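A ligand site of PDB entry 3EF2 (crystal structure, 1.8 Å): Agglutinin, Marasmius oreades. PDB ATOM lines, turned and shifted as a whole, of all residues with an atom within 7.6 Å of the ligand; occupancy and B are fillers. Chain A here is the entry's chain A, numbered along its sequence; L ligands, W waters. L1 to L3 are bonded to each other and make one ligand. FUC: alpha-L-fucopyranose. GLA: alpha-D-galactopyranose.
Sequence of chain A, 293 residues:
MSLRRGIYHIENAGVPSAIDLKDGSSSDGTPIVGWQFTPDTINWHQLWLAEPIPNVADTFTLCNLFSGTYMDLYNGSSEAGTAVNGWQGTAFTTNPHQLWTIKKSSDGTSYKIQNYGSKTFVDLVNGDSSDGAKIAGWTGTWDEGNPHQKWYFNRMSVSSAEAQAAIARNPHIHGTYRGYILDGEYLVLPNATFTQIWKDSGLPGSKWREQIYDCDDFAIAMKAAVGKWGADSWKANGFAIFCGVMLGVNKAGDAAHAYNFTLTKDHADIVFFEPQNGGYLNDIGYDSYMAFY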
ATOM      1  N   ALA A  80     -13.024  23.913 -10.951  1.00  0.00           N
ATOM      2  CA  ALA A  80     -12.903  24.806 -12.108  1.00  0.00           C
ATOM      3  C   ALA A  80     -14.298  25.302 -12.498  1.00  0.00           C
ATOM      4  O   ALA A  80     -15.243  24.510 -12.567  1.00  0.00           O
ATOM      5  CB  ALA A  80     -12.222  24.109 -13.264  1.00  0.00           C
ATOM      6  N   GLY A  81     -14.432  26.615 -12.728  1.00  0.00           N
ATOM      7  CA  GLY A  81     -15.713  27.198 -13.111  1.00  0.00           C
ATOM      8  C   GLY A  81     -16.526  27.791 -11.966  1.00  0.00           C
ATOM      9  O   GLY A  81     -17.660  28.241 -12.165  1.00  0.00           O
ATOM     10  N   LYS A 112      -1.045  37.051 -11.769  1.00  0.00           N
ATOM     11  CA  LYS A 112      -2.105  36.072 -11.569  1.00  0.00           C
ATOM     12  C   LYS A 112      -2.729  36.318 -10.202  1.00  0.00           C
ATOM     13  O   LYS A 112      -2.084  36.847  -9.298  1.00  0.00           O
ATOM     14  CB  LYS A 112      -1.597  34.626 -11.724  1.00  0.00           C
ATOM     15  CG  LYS A 112      -0.828  34.388 -13.053  1.00  0.00           C
ATOM     16  CD  LYS A 112      -0.724  32.868 -13.410  1.00  0.00           C
ATOM     17  CE  LYS A 112      -2.122  32.199 -13.484  1.00  0.00           C
ATOM     18  NZ  LYS A 112      -2.155  31.030 -14.411  1.00  0.00           N
ATOM     19  N   PHE A 121      -7.228  29.989  -9.663  1.00  0.00           N
ATOM     20  CA  PHE A 121      -6.937  31.314 -10.221  1.00  0.00           C
ATOM     21  C   PHE A 121      -8.154  31.991 -10.845  1.00  0.00           C
ATOM     22  O   PHE A 121      -9.037  31.332 -11.404  1.00  0.00           O
ATOM     23  CB  PHE A 121      -5.799  31.227 -11.262  1.00  0.00           C
ATOM     24  CG  PHE A 121      -4.474  30.849 -10.650  1.00  0.00           C
ATOM     25  CD1 PHE A 121      -3.600  31.821 -10.171  1.00  0.00           C
ATOM     26  CD2 PHE A 121      -4.129  29.499 -10.514  1.00  0.00           C
ATOM     27  CE1 PHE A 121      -2.382  31.460  -9.595  1.00  0.00           C
ATOM     28  CE2 PHE A 121      -2.904  29.126  -9.920  1.00  0.00           C
ATOM     29  CZ  PHE A 121      -2.045  30.095  -9.460  1.00  0.00           C
ATOM     30  N   VAL A 122      -8.185  33.317 -10.762  1.00  0.00           N
ATOM     31  CA  VAL A 122      -9.184  34.145 -11.463  1.00  0.00           C
ATOM     32  C   VAL A 122      -9.001  33.987 -12.969  1.00  0.00           C
ATOM     33  O   VAL A 122      -7.928  34.267 -13.516  1.00  0.00           O
ATOM     34  CB  VAL A 122      -9.076  35.645 -11.037  1.00  0.00           C
ATOM     35  CG1 VAL A 122      -9.993  36.548 -11.897  1.00  0.00           C
ATOM     36  CG2 VAL A 122      -9.411  35.769  -9.539  1.00  0.00           C
ATOM     37  N   ASP A 123     -10.062  33.537 -13.638  1.00  0.00           N
ATOM     38  CA  ASP A 123      -9.978  33.112 -15.034  1.00  0.00           C
ATOM     39  C   ASP A 123     -11.109  33.753 -15.858  1.00  0.00           C
ATOM     40  O   ASP A 123     -12.271  33.564 -15.532  1.00  0.00           O
ATOM     41  CB  ASP A 123     -10.045  31.561 -15.093  1.00  0.00           C
ATOM     42  CG  ASP A 123      -9.826  30.995 -16.503  1.00  0.00           C
ATOM     43  OD1 ASP A 123     -10.537  31.405 -17.451  1.00  0.00           O
ATOM     44  OD2 ASP A 123      -8.934  30.118 -16.671  1.00  0.00           O
ATOM     45  N   LEU A 124     -10.758  34.526 -16.896  1.00  0.00           N
ATOM     46  CA  LEU A 124     -11.726  34.999 -17.886  1.00  0.00           C
ATOM     47  C   LEU A 124     -12.054  33.809 -18.800  1.00  0.00           C
ATOM     48  O   LEU A 124     -11.254  33.443 -19.671  1.00  0.00           O
ATOM     49  CB  LEU A 124     -11.186  36.202 -18.698  1.00  0.00           C
ATOM     50  CG  LEU A 124     -12.123  36.849 -19.745  1.00  0.00           C
ATOM     51  CD1 LEU A 124     -13.425  37.428 -19.130  1.00  0.00           C
ATOM     52  CD2 LEU A 124     -11.375  37.927 -20.541  1.00  0.00           C
ATOM     53  N   VAL A 125     -13.226  33.202 -18.570  1.00  0.00           N
ATOM     54  CA  VAL A 125     -13.517  31.876 -19.111  1.00  0.00           C
ATOM     55  C   VAL A 125     -13.472  31.918 -20.647  1.00  0.00           C
ATOM     56  O   VAL A 125     -14.164  32.720 -21.279  1.00  0.00           O
ATOM     57  CB  VAL A 125     -14.833  31.258 -18.546  1.00  0.00           C
ATOM     58  CG1 VAL A 125     -15.074  29.837 -19.146  1.00  0.00           C
ATOM     59  CG2 VAL A 125     -14.768  31.175 -17.010  1.00  0.00           C
ATOM     60  N   ASN A 126     -12.600  31.063 -21.203  1.00  0.00           N
ATOM     61  CA  ASN A 126     -12.393  30.906 -22.649  1.00  0.00           C
ATOM     62  C   ASN A 126     -11.839  32.161 -23.320  1.00  0.00           C
ATOM     63  O   ASN A 126     -11.876  32.272 -24.545  1.00  0.00           O
ATOM     64  CB  ASN A 126     -13.706  30.483 -23.363  1.00  0.00           C
ATOM     65  CG  ASN A 126     -14.068  29.051 -23.086  1.00  0.00           C
ATOM     66  OD1 ASN A 126     -13.191  28.181 -23.037  1.00  0.00           O
ATOM     67  ND2 ASN A 126     -15.369  28.777 -22.930  1.00  0.00           N
ATOM     68  N   GLY A 127     -11.296  33.076 -22.532  1.00  0.00           N
ATOM     69  CA  GLY A 127     -10.788  34.346 -23.092  1.00  0.00           C
ATOM     70  C   GLY A 127     -11.853  35.153 -23.812  1.00  0.00           C
ATOM     71  O   GLY A 127     -11.557  35.889 -24.760  1.00  0.00           O
ATOM     72  N   ASP A 128     -13.096  35.022 -23.345  1.00  0.00           N
ATOM     73  CA  ASP A 128     -14.251  35.635 -24.011  1.00  0.00           C
ATOM     74  C   ASP A 128     -14.196  37.152 -23.797  1.00  0.00           C
ATOM     75  O   ASP A 128     -14.166  37.617 -22.650  1.00  0.00           O
ATOM     76  CB  ASP A 128     -15.530  35.033 -23.398  1.00  0.00           C
ATOM     77  CG  ASP A 128     -16.826  35.527 -24.077  1.00  0.00           C
ATOM     78  OD1 ASP A 128     -16.789  36.407 -24.954  1.00  0.00           O
ATOM     79  OD2 ASP A 128     -17.881  34.980 -23.703  1.00  0.00           O
ATOM     80  N   LYS A 134     -18.286  35.453 -18.285  1.00  0.00           N
ATOM     81  CA  LYS A 134     -18.036  34.874 -16.977  1.00  0.00           C
ATOM     82  C   LYS A 134     -16.572  34.901 -16.548  1.00  0.00           C
ATOM     83  O   LYS A 134     -15.675  34.552 -17.330  1.00  0.00           O
ATOM     84  CB  LYS A 134     -18.506  33.422 -16.956  1.00  0.00           C
ATOM     85  CG  LYS A 134     -18.258  32.741 -15.603  1.00  0.00           C
ATOM     86  CD  LYS A 134     -18.718  31.262 -15.643  1.00  0.00           C
ATOM     87  CE  LYS A 134     -20.244  31.138 -15.526  1.00  0.00           C
ATOM     88  NZ  LYS A 134     -20.747  29.704 -15.508  1.00  0.00           N
ATOM     89  N   ALA A 136     -14.341  33.164 -13.438  1.00  0.00           N
ATOM     90  CA  ALA A 136     -14.514  32.039 -12.546  1.00  0.00           C
ATOM     91  C   ALA A 136     -13.185  31.657 -11.911  1.00  0.00           C
ATOM     92  O   ALA A 136     -12.120  32.012 -12.422  1.00  0.00           O
ATOM     93  CB  ALA A 136     -15.080  30.852 -13.334  1.00  0.00           C
ATOM     94  N   TRP A 138     -10.428  28.872 -11.353  1.00  0.00           N
ATOM     95  CA  TRP A 138     -10.035  27.794 -12.257  1.00  0.00           C
ATOM     96  C   TRP A 138      -8.653  27.230 -11.903  1.00  0.00           C
ATOM     97  O   TRP A 138      -7.751  27.968 -11.434  1.00  0.00           O
ATOM     98  CB  TRP A 138     -10.022  28.306 -13.715  1.00  0.00           C
ATOM     99  CG  TRP A 138     -10.322  27.253 -14.772  1.00  0.00           C
ATOM    100  CD1 TRP A 138      -9.490  26.271 -15.219  1.00  0.00           C
ATOM    101  CD2 TRP A 138     -11.548  27.117 -15.526  1.00  0.00           C
ATOM    102  NE1 TRP A 138     -10.118  25.521 -16.204  1.00  0.00           N
ATOM    103  CE2 TRP A 138     -11.381  26.025 -16.411  1.00  0.00           C
ATOM    104  CE3 TRP A 138     -12.767  27.823 -15.536  1.00  0.00           C
ATOM    105  CZ2 TRP A 138     -12.389  25.606 -17.297  1.00  0.00           C
ATOM    106  CZ3 TRP A 138     -13.769  27.413 -16.413  1.00  0.00           C
ATOM    107  CH2 TRP A 138     -13.576  26.310 -17.274  1.00  0.00           C
ATOM    108  N   THR A 139      -8.508  25.920 -12.123  1.00  0.00           N
ATOM    109  CA  THR A 139      -7.216  25.262 -11.990  1.00  0.00           C
ATOM    110  C   THR A 139      -6.178  25.994 -12.823  1.00  0.00           C
ATOM    111  O   THR A 139      -6.484  26.529 -13.900  1.00  0.00           O
ATOM    112  CB  THR A 139      -7.252  23.774 -12.416  1.00  0.00           C
ATOM    113  OG1 THR A 139      -7.754  23.653 -13.754  1.00  0.00           O
ATOM    114  CG2 THR A 139      -8.120  22.964 -11.494  1.00  0.00           C
ATOM    115  N   GLY A 140      -4.948  26.026 -12.320  1.00  0.00           N
ATOM    116  CA  GLY A 140      -3.864  26.644 -13.055  1.00  0.00           C
ATOM    117  C   GLY A 140      -2.564  26.616 -12.279  1.00  0.00           C
ATOM    118  O   GLY A 140      -2.483  26.084 -11.154  1.00  0.00           O
ATOM    119  N   THR A 141      -1.526  27.195 -12.884  1.00  0.00           N
ATOM    120  CA  THR A 141      -0.212  27.246 -12.251  1.00  0.00           C
ATOM    121  C   THR A 141       0.336  28.692 -12.248  1.00  0.00           C
ATOM    122  O   THR A 141      -0.101  29.539 -13.041  1.00  0.00           O
ATOM    123  CB  THR A 141       0.803  26.320 -12.972  1.00  0.00           C
ATOM    124  OG1 THR A 141       1.136  26.891 -14.229  1.00  0.00           O
ATOM    125  CG2 THR A 141       0.233  24.921 -13.195  1.00  0.00           C
ATOM    126  N   GLU A 144       2.561  29.275 -15.907  1.00  0.00           N
ATOM    127  CA  GLU A 144       2.079  29.039 -17.274  1.00  0.00           C
ATOM    128  C   GLU A 144       1.703  30.341 -17.981  1.00  0.00           C
ATOM    129  O   GLU A 144       1.404  31.357 -17.325  1.00  0.00           O
ATOM    130  CB  GLU A 144       0.904  28.086 -17.291  1.00  0.00           C
ATOM    131  CG  GLU A 144      -0.290  28.628 -16.499  1.00  0.00           C
ATOM    132  CD  GLU A 144      -1.409  27.619 -16.405  1.00  0.00           C
ATOM    133  OE1 GLU A 144      -1.370  26.577 -17.127  1.00  0.00           O
ATOM    134  OE2 GLU A 144      -2.346  27.865 -15.627  1.00  0.00           O
ATOM    135  N   GLY A 145       1.725  30.303 -19.309  1.00  0.00           N
ATOM    136  CA  GLY A 145       1.471  31.489 -20.132  1.00  0.00           C
ATOM    137  C   GLY A 145       0.014  31.880 -20.318  1.00  0.00           C
ATOM    138  O   GLY A 145      -0.267  32.969 -20.814  1.00  0.00           O
ATOM    139  N   ASN A 146      -0.904  30.965 -19.952  1.00  0.00           N
ATOM    140  CA  ASN A 146      -2.347  31.104 -20.232  1.00  0.00           C
ATOM    141  C   ASN A 146      -2.900  32.515 -19.985  1.00  0.00           C
ATOM    142  O   ASN A 146      -3.021  32.949 -18.816  1.00  0.00           O
ATOM    143  CB  ASN A 146      -3.134  30.053 -19.421  1.00  0.00           C
ATOM    144  CG  ASN A 146      -4.652  30.082 -19.693  1.00  0.00           C
ATOM    145  OD1 ASN A 146      -5.139  30.824 -20.560  1.00  0.00           O
ATOM    146  ND2 ASN A 146      -5.399  29.278 -18.926  1.00  0.00           N
ATOM    147  N   PRO A 147      -3.218  33.255 -21.060  1.00  0.00           N
ATOM    148  CA  PRO A 147      -3.690  34.644 -20.867  1.00  0.00           C
ATOM    149  C   PRO A 147      -5.077  34.777 -20.229  1.00  0.00           C
ATOM    150  O   PRO A 147      -5.434  35.880 -19.791  1.00  0.00           O
ATOM    151  CB  PRO A 147      -3.668  35.246 -22.284  1.00  0.00           C
ATOM    152  CG  PRO A 147      -3.786  34.065 -23.200  1.00  0.00           C
ATOM    153  CD  PRO A 147      -3.171  32.887 -22.495  1.00  0.00           C
ATOM    154  N   HIS A 148      -5.860  33.694 -20.209  1.00  0.00           N
ATOM    155  CA  HIS A 148      -7.158  33.704 -19.511  1.00  0.00           C
ATOM    156  C   HIS A 148      -6.987  34.037 -18.019  1.00  0.00           C
ATOM    157  O   HIS A 148      -7.920  34.526 -17.378  1.00  0.00           O
ATOM    158  CB  HIS A 148      -7.906  32.364 -19.652  1.00  0.00           C
ATOM    159  CG  HIS A 148      -8.127  31.920 -21.076  1.00  0.00           C
ATOM    160  ND1 HIS A 148      -8.700  30.711 -21.389  1.00  0.00           N
ATOM    161  CD2 HIS A 148      -7.885  32.542 -22.255  1.00  0.00           C
ATOM    162  CE1 HIS A 148      -8.790  30.595 -22.702  1.00  0.00           C
ATOM    163  NE2 HIS A 148      -8.298  31.694 -23.253  1.00  0.00           N
ATOM    164  N   GLN A 149      -5.794  33.762 -17.495  1.00  0.00           N
ATOM    165  CA  GLN A 149      -5.534  33.924 -16.066  1.00  0.00           C
ATOM    166  C   GLN A 149      -4.483  34.998 -15.755  1.00  0.00           C
ATOM    167  O   GLN A 149      -3.984  35.075 -14.630  1.00  0.00           O
ATOM    168  CB  GLN A 149      -5.110  32.579 -15.466  1.00  0.00           C
ATOM    169  CG  GLN A 149      -6.205  31.523 -15.569  1.00  0.00           C
ATOM    170  CD  GLN A 149      -5.820  30.207 -14.925  1.00  0.00           C
ATOM    171  OE1 GLN A 149      -4.719  30.072 -14.352  1.00  0.00           O
ATOM    172  NE2 GLN A 149      -6.708  29.219 -15.006  1.00  0.00           N
HETATM  173  C1  FUC L   1      -5.537  26.291 -21.962  1.00  0.00           C
HETATM  174  C2  FUC L   1      -4.658  25.073 -22.241  1.00  0.00           C
HETATM  175  C3  FUC L   1      -5.390  24.113 -23.189  1.00  0.00           C
HETATM  176  C4  FUC L   1      -5.691  24.855 -24.459  1.00  0.00           C
HETATM  177  C5  FUC L   1      -6.505  26.126 -24.134  1.00  0.00           C
HETATM  178  C6  FUC L   1      -6.934  26.942 -25.354  1.00  0.00           C
HETATM  179  O2  FUC L   1      -4.311  24.425 -21.053  1.00  0.00           O
HETATM  180  O3  FUC L   1      -4.578  22.977 -23.451  1.00  0.00           O
HETATM  181  O4  FUC L   1      -4.458  25.202 -25.036  1.00  0.00           O
HETATM  182  O5  FUC L   1      -5.813  26.948 -23.180  1.00  0.00           O
HETATM  183  C1  GLA L   2      -8.900  26.882 -21.588  1.00  0.00           C
HETATM  184  C2  GLA L   2      -7.582  26.778 -20.808  1.00  0.00           C
HETATM  185  C3  GLA L   2      -7.813  26.532 -19.315  1.00  0.00           C
HETATM  186  C4  GLA L   2      -8.773  27.602 -18.752  1.00  0.00           C
HETATM  187  C5  GLA L   2     -10.064  27.561 -19.571  1.00  0.00           C
HETATM  188  C6  GLA L   2     -11.145  28.518 -19.052  1.00  0.00           C
HETATM  189  O1  GLA L   2      -9.507  25.585 -21.622  1.00  0.00           O
HETATM  190  O2  GLA L   2      -6.725  25.847 -21.326  1.00  0.00           O
HETATM  191  O3  GLA L   2      -6.540  26.511 -18.659  1.00  0.00           O
HETATM  192  O4  GLA L   2      -8.138  28.885 -18.804  1.00  0.00           O
HETATM  193  O5  GLA L   2      -9.805  27.804 -20.981  1.00  0.00           O
HETATM  194  O6  GLA L   2     -10.858  29.844 -19.530  1.00  0.00           O
HETATM  195  C1  GLA L   3      -6.540  26.230 -17.254  1.00  0.00           C
HETATM  196  C2  GLA L   3      -5.090  26.075 -16.785  1.00  0.00           C
HETATM  197  C3  GLA L   3      -4.490  24.766 -17.323  1.00  0.00           C
HETATM  198  C4  GLA L   3      -5.393  23.566 -16.974  1.00  0.00           C
HETATM  199  C5  GLA L   3      -6.803  23.845 -17.515  1.00  0.00           C
HETATM  200  C6  GLA L   3      -7.815  22.723 -17.215  1.00  0.00           C
HETATM  201  O2  GLA L   3      -4.368  27.274 -17.160  1.00  0.00           O
HETATM  202  O3  GLA L   3      -3.200  24.580 -16.768  1.00  0.00           O
HETATM  203  O4  GLA L   3      -5.462  23.361 -15.544  1.00  0.00           O
HETATM  204  O5  GLA L   3      -7.294  25.071 -16.959  1.00  0.00           O
HETATM  205  O6  GLA L   3      -9.085  23.028 -17.810  1.00  0.00           O
HETATM  206  O   HOH W   1     -11.371  22.394 -16.233  1.00  0.00           O
HETATM  207  O   HOH W   2      -5.016  25.203 -28.089  1.00  0.00           O
HETATM  208  O   HOH W   3      -5.811  22.396 -20.625  1.00  0.00           O
HETATM  209  O   HOH W   4      -2.790  26.516 -19.680  1.00  0.00           O
HETATM  210  O   HOH W   5      -3.407  22.094 -20.818  1.00  0.00           O
HETATM  211  O   HOH W   6      -2.904  23.245 -13.934  1.00  0.00           O
HETATM  212  O   HOH W   7     -10.534  28.162 -24.392  1.00  0.00           O
HETATM  213  O   HOH W   8      -5.365  29.668 -23.125  1.00  0.00           O
HETATM  214  O   HOH W   9      -1.354  22.750 -22.225  1.00  0.00           O
HETATM  215  O   HOH W  10      -8.318  22.955 -20.701  1.00  0.00           O
HETATM  216  O   HOH W  11      -4.894  20.796 -14.779  1.00  0.00           O
HETATM  217  O   HOH W  12      -2.106  22.845 -18.737  1.00  0.00           O
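Water W8 lies within hydrogen-bond range of O5 of FUC L1 (2.8 Å) and OD1 of Asn 146 (2.8 Å).
Water W1 bridges O6 of GLA L3 and NE1 of Trp 138.
Water W4 lies within hydrogen-bond range of the side-chain carboxylate of Glu 144 (2.9 Å) and an oxygen (O2) of FUC L1 (2.9 Å).
The backbone NH (N) of Val 125 is in hydrogen-bond range of the side-chain carboxylate (OD1) of Asp 123.
The side-chain carboxylate of Asp 123 is in hydrogen-bond range of the side-chain amide nitrogen of Gln 149 (2.9 Å).
N of Asp 123 is in hydrogen-bond range of O of Ala 136 (2.8 Å).
The side-chain carboxylate (OE2) of Glu 144 sits close to the side-chain amide oxygen (OE1) of Gln 149.
The side-chain carboxylate (OE2) of Glu 144 lies within hydrogen-bond range of the backbone NH (N) of Thr 141, 2.9 Å away.
The side-chain amide nitrogen (NE2) of Gln 149 is in hydrogen-bond range of the backbone carbonyl oxygen (O) of Thr 139 (2.9 Å).
A ring nitrogen (NE2) of His 148 sits at hydrogen-bond distance from the backbone NH of Gly 127, at 3.4 Å.
The side-chain amino group of Lys 112 lies within hydrogen-bond range of the side-chain amide oxygen of Gln 149.
OD2 of Asp 123 is in hydrogen-bond range of O4 of GLA L2, 2.6 Å away.
The side-chain carboxylate (OE2) of Glu 144 is in hydrogen-bond range of an oxygen (O2) of GLA L3 (2.6 Å).
The backbone NH of Asn 126 sits at hydrogen-bond distance from an oxygen (O6) of GLA L2 (2.7 Å).
The side-chain amide nitrogen (ND2) of Asn 146 lies within hydrogen-bond range of an oxygen (O4) of GLA L2, 2.8 Å away.
O4 of GLA L3 sits at hydrogen-bond distance from OG1 of Thr 139 (2.9 Å).
The indole nitrogen (NE1) of Trp 138 lies within hydrogen-bond range of an oxygen (O5) of GLA L3 (3.0 Å).
ND1 of His 148 lies within hydrogen-bond range of O6 of GLA L2 (3.0 Å).
Residues that only touch the ligand: Val 125 (3.4 Å), Leu 124 (3.6 Å), Gln 149 (3.7 Å) and Gly 140 (3.97 Å).
Hydrophobic or aromatic side chains that line the ligand: Trp 138 and His 148.
11 residues have an atom within 4 Å of the ligand: Asp 123, Leu 124, Val 125, Asn 126, Trp 138, Thr 139, Gly 140, Glu 144, Asn 146, His 148 and Gln 149.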
